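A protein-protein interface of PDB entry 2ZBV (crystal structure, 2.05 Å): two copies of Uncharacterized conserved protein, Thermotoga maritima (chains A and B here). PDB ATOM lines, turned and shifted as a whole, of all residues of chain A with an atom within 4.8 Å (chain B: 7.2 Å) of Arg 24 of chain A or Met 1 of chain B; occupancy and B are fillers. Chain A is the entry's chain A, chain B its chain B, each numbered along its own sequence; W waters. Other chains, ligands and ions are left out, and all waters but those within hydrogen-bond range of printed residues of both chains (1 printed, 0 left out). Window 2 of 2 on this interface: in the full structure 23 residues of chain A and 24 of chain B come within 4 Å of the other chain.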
ATOM      1  N   ALA A  20      14.864  -0.361 -27.101  1.00  0.00           N
ATOM      2  CA  ALA A  20      13.601  -0.247 -26.381  1.00  0.00           C
ATOM      3  C   ALA A  20      12.547   0.327 -27.320  1.00  0.00           C
ATOM      4  O   ALA A  20      11.413  -0.145 -27.348  1.00  0.00           O
ATOM      5  CB  ALA A  20      13.767   0.648 -25.161  1.00  0.00           C
ATOM      6  N   VAL A  21      12.928   1.335 -28.100  1.00  0.00           N
ATOM      7  CA  VAL A  21      12.005   1.955 -29.041  1.00  0.00           C
ATOM      8  C   VAL A  21      11.549   0.943 -30.090  1.00  0.00           C
ATOM      9  O   VAL A  21      10.371   0.885 -30.440  1.00  0.00           O
ATOM     10  CB  VAL A  21      12.663   3.157 -29.748  1.00  0.00           C
ATOM     11  CG1 VAL A  21      11.829   3.576 -30.951  1.00  0.00           C
ATOM     12  CG2 VAL A  21      12.800   4.325 -28.764  1.00  0.00           C
ATOM     13  N   ILE A  22      12.489   0.147 -30.591  1.00  0.00           N
ATOM     14  CA  ILE A  22      12.178  -0.863 -31.587  1.00  0.00           C
ATOM     15  C   ILE A  22      11.219  -1.912 -31.023  1.00  0.00           C
ATOM     16  O   ILE A  22      10.213  -2.246 -31.653  1.00  0.00           O
ATOM     17  CB  ILE A  22      13.461  -1.573 -32.074  1.00  0.00           C
ATOM     18  CG1 ILE A  22      14.338  -0.578 -32.839  1.00  0.00           C
ATOM     19  CG2 ILE A  22      13.094  -2.783 -32.956  1.00  0.00           C
ATOM     20  CD1 ILE A  22      15.666  -1.161 -33.296  1.00  0.00           C
ATOM     21  N   LYS A  23      11.534  -2.414 -29.831  1.00  0.00           N
ATOM     22  CA  LYS A  23      10.728  -3.439 -29.171  1.00  0.00           C
ATOM     23  C   LYS A  23       9.356  -2.948 -28.716  1.00  0.00           C
ATOM     24  O   LYS A  23       8.448  -3.751 -28.485  1.00  0.00           O
ATOM     25  CB  LYS A  23      11.486  -4.003 -27.969  1.00  0.00           C
ATOM     26  CG  LYS A  23      12.672  -4.879 -28.336  1.00  0.00           C
ATOM     27  CD  LYS A  23      12.206  -6.190 -28.956  1.00  0.00           C
ATOM     28  CE  LYS A  23      13.354  -7.174 -29.105  1.00  0.00           C
ATOM     29  NZ  LYS A  23      12.858  -8.513 -29.528  1.00  0.00           N
ATOM     30  N   ARG A  24       9.215  -1.634 -28.564  1.00  0.00           N
ATOM     31  CA  ARG A  24       7.939  -1.056 -28.156  1.00  0.00           C
ATOM     32  C   ARG A  24       7.041  -1.109 -29.380  1.00  0.00           C
ATOM     33  O   ARG A  24       5.847  -1.387 -29.277  1.00  0.00           O
ATOM     34  CB  ARG A  24       8.118   0.398 -27.689  1.00  0.00           C
ATOM     35  CG  ARG A  24       8.919   0.533 -26.399  1.00  0.00           C
ATOM     36  CD  ARG A  24       9.197   1.989 -26.014  1.00  0.00           C
ATOM     37  NE  ARG A  24       7.984   2.679 -25.579  1.00  0.00           N
ATOM     38  CZ  ARG A  24       7.964   3.875 -24.994  1.00  0.00           C
ATOM     39  NH1 ARG A  24       9.097   4.531 -24.766  1.00  0.00           N
ATOM     40  NH2 ARG A  24       6.807   4.415 -24.633  1.00  0.00           N
ATOM     41  N   ILE A  25       7.637  -0.850 -30.540  1.00  0.00           N
ATOM     42  CA  ILE A  25       6.909  -0.877 -31.800  1.00  0.00           C
ATOM     43  C   ILE A  25       6.591  -2.317 -32.188  1.00  0.00           C
ATOM     44  O   ILE A  25       5.458  -2.637 -32.530  1.00  0.00           O
ATOM     45  CB  ILE A  25       7.727  -0.221 -32.918  1.00  0.00           C
ATOM     46  CG1 ILE A  25       7.778   1.289 -32.691  1.00  0.00           C
ATOM     47  CG2 ILE A  25       7.114  -0.531 -34.276  1.00  0.00           C
ATOM     48  CD1 ILE A  25       8.619   2.011 -33.700  1.00  0.00           C
ATOM     49  N   ASN A  26       7.597  -3.183 -32.120  1.00  0.00           N
ATOM     50  CA  ASN A  26       7.424  -4.589 -32.457  1.00  0.00           C
ATOM     51  C   ASN A  26       8.084  -5.470 -31.401  1.00  0.00           C
ATOM     52  O   ASN A  26       9.292  -5.694 -31.431  1.00  0.00           O
ATOM     53  CB  ASN A  26       8.041  -4.890 -33.822  1.00  0.00           C
ATOM     54  CG  ASN A  26       7.892  -6.352 -34.220  1.00  0.00           C
ATOM     55  OD1 ASN A  26       8.507  -6.810 -35.186  1.00  0.00           O
ATOM     56  ND2 ASN A  26       7.069  -7.091 -33.478  1.00  0.00           N
ATOM     57  N   PRO A  27       7.292  -5.987 -30.453  1.00  0.00           N
ATOM     58  CA  PRO A  27       7.840  -6.843 -29.397  1.00  0.00           C
ATOM     59  C   PRO A  27       8.487  -8.104 -29.948  1.00  0.00           C
ATOM     60  O   PRO A  27       9.282  -8.752 -29.267  1.00  0.00           O
ATOM     61  CB  PRO A  27       6.617  -7.156 -28.535  1.00  0.00           C
ATOM     62  CG  PRO A  27       5.746  -5.946 -28.728  1.00  0.00           C
ATOM     63  CD  PRO A  27       5.865  -5.702 -30.214  1.00  0.00           C
ATOM     64  N   TYR A 118       9.314   8.080 -33.631  1.00  0.00           N
ATOM     65  CA  TYR A 118       9.095   7.692 -32.242  1.00  0.00           C
ATOM     66  C   TYR A 118       8.496   8.891 -31.509  1.00  0.00           C
ATOM     67  O   TYR A 118       7.706   8.733 -30.581  1.00  0.00           O
ATOM     68  CB  TYR A 118      10.431   7.257 -31.615  1.00  0.00           C
ATOM     69  CG  TYR A 118      10.499   7.240 -30.099  1.00  0.00           C
ATOM     70  CD1 TYR A 118       9.598   6.496 -29.336  1.00  0.00           C
ATOM     71  CD2 TYR A 118      11.502   7.947 -29.428  1.00  0.00           C
ATOM     72  CE1 TYR A 118       9.700   6.455 -27.930  1.00  0.00           C
ATOM     73  CE2 TYR A 118      11.613   7.917 -28.041  1.00  0.00           C
ATOM     74  CZ  TYR A 118      10.712   7.170 -27.296  1.00  0.00           C
ATOM     75  OH  TYR A 118      10.844   7.138 -25.925  1.00  0.00           O
ATOM     76  N   MET B   1       9.061  -5.633 -20.266  1.00  0.00           N
ATOM     77  CA  MET B   1      10.486  -5.920 -20.588  1.00  0.00           C
ATOM     78  C   MET B   1      11.367  -5.531 -19.403  1.00  0.00           C
ATOM     79  O   MET B   1      10.908  -4.863 -18.476  1.00  0.00           O
ATOM     80  CB  MET B   1      10.905  -5.158 -21.854  1.00  0.00           C
ATOM     81  CG  MET B   1      10.638  -3.657 -21.806  1.00  0.00           C
ATOM     82  SD  MET B   1      11.426  -2.694 -23.308  1.00  0.00           S
ATOM     83  CE  MET B   1       9.926  -2.747 -24.547  1.00  0.00           C
ATOM     84  N   ILE B   2      12.630  -5.951 -19.431  1.00  0.00           N
ATOM     85  CA  ILE B   2      13.560  -5.660 -18.340  1.00  0.00           C
ATOM     86  C   ILE B   2      14.748  -4.813 -18.781  1.00  0.00           C
ATOM     87  O   ILE B   2      15.446  -5.163 -19.735  1.00  0.00           O
ATOM     88  CB  ILE B   2      14.114  -6.978 -17.716  1.00  0.00           C
ATOM     89  CG1 ILE B   2      12.966  -7.822 -17.149  1.00  0.00           C
ATOM     90  CG2 ILE B   2      15.134  -6.661 -16.619  1.00  0.00           C
ATOM     91  CD1 ILE B   2      13.417  -9.167 -16.588  1.00  0.00           C
ATOM     92  N   GLY B   3      14.967  -3.695 -18.092  1.00  0.00           N
ATOM     93  CA  GLY B   3      16.106  -2.844 -18.398  1.00  0.00           C
ATOM     94  C   GLY B   3      17.222  -3.290 -17.468  1.00  0.00           C
ATOM     95  O   GLY B   3      17.073  -3.211 -16.251  1.00  0.00           O
ATOM     96  N   ALA B  29      11.195 -13.770 -21.468  1.00  0.00           N
ATOM     97  CA  ALA B  29      11.663 -12.488 -20.947  1.00  0.00           C
ATOM     98  C   ALA B  29      12.449 -11.712 -22.001  1.00  0.00           C
ATOM     99  O   ALA B  29      13.318 -12.270 -22.676  1.00  0.00           O
ATOM    100  CB  ALA B  29      12.528 -12.703 -19.714  1.00  0.00           C
ATOM    101  N   GLU B  30      12.124 -10.429 -22.143  1.00  0.00           N
ATOM    102  CA  GLU B  30      12.795  -9.540 -23.089  1.00  0.00           C
ATOM    103  C   GLU B  30      13.787  -8.687 -22.297  1.00  0.00           C
ATOM    104  O   GLU B  30      13.396  -7.749 -21.605  1.00  0.00           O
ATOM    105  CB  GLU B  30      11.768  -8.634 -23.780  1.00  0.00           C
ATOM    106  CG  GLU B  30      12.365  -7.628 -24.754  1.00  0.00           C
ATOM    107  CD  GLU B  30      13.129  -8.285 -25.889  1.00  0.00           C
ATOM    108  OE1 GLU B  30      12.515  -9.065 -26.650  1.00  0.00           O
ATOM    109  OE2 GLU B  30      14.345  -8.018 -26.019  1.00  0.00           O
ATOM    110  N   ILE B  31      15.070  -9.013 -22.401  1.00  0.00           N
ATOM    111  CA  ILE B  31      16.100  -8.282 -21.664  1.00  0.00           C
ATOM    112  C   ILE B  31      16.846  -7.262 -22.519  1.00  0.00           C
ATOM    113  O   ILE B  31      17.491  -7.619 -23.508  1.00  0.00           O
ATOM    114  CB  ILE B  31      17.132  -9.259 -21.075  1.00  0.00           C
ATOM    115  CG1 ILE B  31      16.410 -10.363 -20.307  1.00  0.00           C
ATOM    116  CG2 ILE B  31      18.100  -8.515 -20.155  1.00  0.00           C
ATOM    117  CD1 ILE B  31      17.308 -11.518 -19.900  1.00  0.00           C
ATOM    118  N   ILE B  32      16.756  -5.993 -22.134  1.00  0.00           N
ATOM    119  CA  ILE B  32      17.444  -4.933 -22.853  1.00  0.00           C
ATOM    120  C   ILE B  32      18.528  -4.337 -21.965  1.00  0.00           C
ATOM    121  O   ILE B  32      18.249  -3.793 -20.898  1.00  0.00           O
ATOM    122  CB  ILE B  32      16.480  -3.807 -23.286  1.00  0.00           C
ATOM    123  CG1 ILE B  32      15.383  -4.390 -24.181  1.00  0.00           C
ATOM    124  CG2 ILE B  32      17.255  -2.713 -24.046  1.00  0.00           C
ATOM    125  CD1 ILE B  32      14.503  -3.357 -24.826  1.00  0.00           C
ATOM    126  N   SER B  54      15.677   5.381 -18.576  1.00  0.00           N
ATOM    127  CA  SER B  54      14.287   5.075 -18.214  1.00  0.00           C
ATOM    128  C   SER B  54      13.252   5.956 -18.908  1.00  0.00           C
ATOM    129  O   SER B  54      12.089   5.565 -19.033  1.00  0.00           O
ATOM    130  CB  SER B  54      14.094   5.172 -16.692  1.00  0.00           C
ATOM    131  OG  SER B  54      14.203   6.512 -16.241  1.00  0.00           O
ATOM    132  N   LEU B  55      13.667   7.136 -19.357  1.00  0.00           N
ATOM    133  CA  LEU B  55      12.763   8.052 -20.044  1.00  0.00           C
ATOM    134  C   LEU B  55      12.284   7.480 -21.378  1.00  0.00           C
ATOM    135  O   LEU B  55      11.234   7.869 -21.881  1.00  0.00           O
ATOM    136  CB  LEU B  55      13.457   9.400 -20.292  1.00  0.00           C
ATOM    137  CG  LEU B  55      13.664  10.326 -19.087  1.00  0.00           C
ATOM    138  CD1 LEU B  55      14.662  11.414 -19.448  1.00  0.00           C
ATOM    139  CD2 LEU B  55      12.315  10.945 -18.658  1.00  0.00           C
ATOM    140  N   ASP B  56      13.048   6.554 -21.950  1.00  0.00           N
ATOM    141  CA  ASP B  56      12.665   5.978 -23.230  1.00  0.00           C
ATOM    142  C   ASP B  56      12.099   4.561 -23.145  1.00  0.00           C
ATOM    143  O   ASP B  56      11.830   3.928 -24.164  1.00  0.00           O
ATOM    144  CB  ASP B  56      13.844   6.021 -24.205  1.00  0.00           C
ATOM    145  CG  ASP B  56      14.170   7.438 -24.658  1.00  0.00           C
ATOM    146  OD1 ASP B  56      13.241   8.163 -25.072  1.00  0.00           O
ATOM    147  OD2 ASP B  56      15.355   7.824 -24.610  1.00  0.00           O
ATOM    148  N   PHE B  57      11.927   4.072 -21.925  1.00  0.00           N
ATOM    149  CA  PHE B  57      11.350   2.754 -21.701  1.00  0.00           C
ATOM    150  C   PHE B  57       9.885   2.992 -21.352  1.00  0.00           C
ATOM    151  O   PHE B  57       9.542   3.990 -20.723  1.00  0.00           O
ATOM    152  CB  PHE B  57      12.057   2.051 -20.542  1.00  0.00           C
ATOM    153  CG  PHE B  57      13.290   1.301 -20.949  1.00  0.00           C
ATOM    154  CD1 PHE B  57      13.241  -0.076 -21.163  1.00  0.00           C
ATOM    155  CD2 PHE B  57      14.504   1.957 -21.099  1.00  0.00           C
ATOM    156  CE1 PHE B  57      14.384  -0.788 -21.516  1.00  0.00           C
ATOM    157  CE2 PHE B  57      15.659   1.254 -21.456  1.00  0.00           C
ATOM    158  CZ  PHE B  57      15.596  -0.126 -21.664  1.00  0.00           C
ATOM    159  N   PRO B  58       8.999   2.078 -21.759  1.00  0.00           N
ATOM    160  CA  PRO B  58       7.582   2.268 -21.449  1.00  0.00           C
ATOM    161  C   PRO B  58       7.230   2.034 -19.979  1.00  0.00           C
ATOM    162  O   PRO B  58       8.051   1.553 -19.196  1.00  0.00           O
ATOM    163  CB  PRO B  58       6.899   1.256 -22.363  1.00  0.00           C
ATOM    164  CG  PRO B  58       7.886   0.116 -22.379  1.00  0.00           C
ATOM    165  CD  PRO B  58       9.222   0.837 -22.524  1.00  0.00           C
ATOM    166  N   PRO B  59       6.006   2.411 -19.582  1.00  0.00           N
ATOM    167  CA  PRO B  59       5.589   2.199 -18.193  1.00  0.00           C
ATOM    168  C   PRO B  59       5.467   0.688 -18.004  1.00  0.00           C
ATOM    169  O   PRO B  59       5.306  -0.044 -18.981  1.00  0.00           O
ATOM    170  CB  PRO B  59       4.240   2.918 -18.121  1.00  0.00           C
ATOM    171  CG  PRO B  59       3.732   2.850 -19.542  1.00  0.00           C
ATOM    172  CD  PRO B  59       4.983   3.163 -20.331  1.00  0.00           C
ATOM    173  N   SER B  60       5.543   0.227 -16.759  1.00  0.00           N
ATOM    174  CA  SER B  60       5.472  -1.194 -16.441  1.00  0.00           C
ATOM    175  C   SER B  60       6.797  -1.902 -16.735  1.00  0.00           C
ATOM    176  O   SER B  60       6.899  -3.127 -16.647  1.00  0.00           O
ATOM    177  CB  SER B  60       4.326  -1.866 -17.206  1.00  0.00           C
ATOM    178  OG  SER B  60       3.068  -1.375 -16.759  1.00  0.00           O
ATOM    179  N   THR B  61       7.818  -1.128 -17.086  1.00  0.00           N
ATOM    180  CA  THR B  61       9.124  -1.714 -17.353  1.00  0.00           C
ATOM    181  C   THR B  61       9.764  -2.066 -16.012  1.00  0.00           C
ATOM    182  O   THR B  61       9.634  -1.325 -15.033  1.00  0.00           O
ATOM    183  CB  THR B  61      10.057  -0.729 -18.111  1.00  0.00           C
ATOM    184  OG1 THR B  61       9.594  -0.560 -19.458  1.00  0.00           O
ATOM    185  CG2 THR B  61      11.487  -1.258 -18.133  1.00  0.00           C
ATOM    186  N   VAL B  62      10.427  -3.214 -15.959  1.00  0.00           N
ATOM    187  CA  VAL B  62      11.100  -3.630 -14.743  1.00  0.00           C
ATOM    188  C   VAL B  62      12.597  -3.418 -14.941  1.00  0.00           C
ATOM    189  O   VAL B  62      13.191  -3.989 -15.856  1.00  0.00           O
ATOM    190  CB  VAL B  62      10.850  -5.117 -14.430  1.00  0.00           C
ATOM    191  CG1 VAL B  62      11.630  -5.514 -13.191  1.00  0.00           C
ATOM    192  CG2 VAL B  62       9.350  -5.365 -14.225  1.00  0.00           C
ATOM    193  N   PHE B  63      13.202  -2.602 -14.084  1.00  0.00           N
ATOM    194  CA  PHE B  63      14.631  -2.332 -14.183  1.00  0.00           C
ATOM    195  C   PHE B  63      15.431  -3.131 -13.169  1.00  0.00           C
ATOM    196  O   PHE B  63      15.141  -3.103 -11.974  1.00  0.00           O
ATOM    197  CB  PHE B  63      14.896  -0.842 -13.974  1.00  0.00           C
ATOM    198  CG  PHE B  63      14.360   0.025 -15.072  1.00  0.00           C
ATOM    199  CD1 PHE B  63      15.133   0.302 -16.193  1.00  0.00           C
ATOM    200  CD2 PHE B  63      13.082   0.569 -14.984  1.00  0.00           C
ATOM    201  CE1 PHE B  63      14.640   1.117 -17.215  1.00  0.00           C
ATOM    202  CE2 PHE B  63      12.582   1.382 -15.997  1.00  0.00           C
ATOM    203  CZ  PHE B  63      13.363   1.658 -17.115  1.00  0.00           C
ATOM    204  N   ALA B 136      13.433  -9.746 -10.463  1.00  0.00           N
ATOM    205  CA  ALA B 136      13.068  -8.918 -11.603  1.00  0.00           C
ATOM    206  C   ALA B 136      12.324  -9.771 -12.626  1.00  0.00           C
ATOM    207  O   ALA B 136      11.356  -9.321 -13.234  1.00  0.00           O
ATOM    208  CB  ALA B 136      14.314  -8.315 -12.232  1.00  0.00           C
ATOM    209  N   ASP B 140       8.490  -9.139 -13.773  1.00  0.00           N
ATOM    210  CA  ASP B 140       8.247  -8.976 -15.200  1.00  0.00           C
ATOM    211  C   ASP B 140       7.207  -9.983 -15.698  1.00  0.00           C
ATOM    212  O   ASP B 140       6.630  -9.802 -16.771  1.00  0.00           O
ATOM    213  CB  ASP B 140       9.546  -9.167 -15.982  1.00  0.00           C
ATOM    214  CG  ASP B 140       9.381  -8.867 -17.458  1.00  0.00           C
ATOM    215  OD1 ASP B 140       8.999  -7.729 -17.790  1.00  0.00           O
ATOM    216  OD2 ASP B 140       9.637  -9.764 -18.287  1.00  0.00           O
HETATM  217  O   HOH W   1       9.910  -8.288 -26.577  1.00  0.00           O
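OH of Tyr 118 of chain A sits at hydrogen-bond distance from OD1 of Asp 56 of chain B, at 2.7 Å.
NH1 of Arg 24 of chain A lies within hydrogen-bond range of O of Asp 56 of chain B, 2.9 Å away.
The side-chain amino group of Lys 23 of chain A is in salt-bridge range of the side-chain carboxylate of Glu 30 of chain B (3.0 Å).
Ala 20 of chain A touches Ile 32 of chain B (CA to CD1, 3.6 Å).
Asp 56 of chain B touches Ala 20 of chain A.
CB of Ala 20 of chain A touches CE1 of Phe 57 of chain B (3.97 Å).
CB of Lys 23 of chain A touches CE of Met 1 of chain B, at 3.96 Å.
CG of Arg 24 of chain A touches CE of Met 1 of chain B, at 3.9 Å.
Arg 24 of chain A touches Phe 57 of chain B.
CD of Pro 58 of chain B touches CD of Arg 24 of chain A, 3.7 Å away.
Of the 9 printed residues of chain A, 4 touch a printed residue of chain B.
Printed residues of chain A that touch a printed residue of chain B: Ala 20, Lys 23, Arg 24 and Tyr 118.
Of the 19 printed residues of chain B, 6 touch a printed residue of chain A.
Hydrophobic or aromatic side chains of chain B that line the printed part of chain A: Met 1, Ile 32, Phe 57 and Pro 58.
Among the printed residues, 10 pairs touch across the chains.
Water W1 lies within hydrogen-bond range of the side-chain carboxylate (OE1) of Glu 30 of chain B and the backbone carbonyl oxygen (O) of Pro 27 of chain A.
The backbone NH (N) of Val 62 of chain B is in hydrogen-bond range of the backbone carbonyl oxygen (O) of Met 1 of chain B (3.0 Å).
The side-chain hydroxyl (OG1) of Thr 61 of chain B lies within hydrogen-bond range of the backbone carbonyl oxygen (O) of Pro 58 of chain B, 2.6 Å away.
The side-chain hydroxyl of Tyr 118 of chain A is in hydrogen-bond range of the guanidinium group of Arg 24 of chain A.
The side-chain carboxylate of Asp 140 of chain B sits at hydrogen-bond distance from the backbone NH of Met 1 of chain B.
N of Ile 32 of chain B sits at hydrogen-bond distance from O of Ile 2 of chain B, at 2.9 Å.
The backbone carbonyl oxygen of Glu 30 of chain B lies within hydrogen-bond range of the backbone NH of Ile 2 of chain B (2.9 Å).
Arg 24 of chain A touches just these residues of chain B: Met 1, Asp 56, Phe 57 and Pro 58.
Met 1 of chain B touches just these residues of chain A: Lys 23 (3.96 Å) and Arg 24 (3.9 Å).
Of the printed residues of chain A, Pro 58 of chain B touches Arg 24.
Of the printed residues of chain A, Phe 57 of chain B touches Ala 20 (3.97 Å) and Arg 24 (3.8 Å).
Of the printed residues of chain B, Tyr 118 of chain A touches Asp 56.
Of the printed residues of chain A, Ile 32 of chain B touches Ala 20 (3.6 Å).
Of the printed residues of chain A, Glu 30 of chain B touches Lys 23.
Phe 63 of chain B touches none of the printed residues of chain A.
Thr 61 of chain B touches none of the printed residues of chain A.
The nearest residue of chain B that does not touch Arg 24 of chain A is Pro 59 of chain B (4.8 Å).
The nearest residue of chain A that does not touch Met 1 of chain B is Ala 20 of chain A (4.1 Å).
No position is printed for both chains.
Of the 10 pairs that touch across the chains among the printed residues, none has its exchanged pair printed and touching as well.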
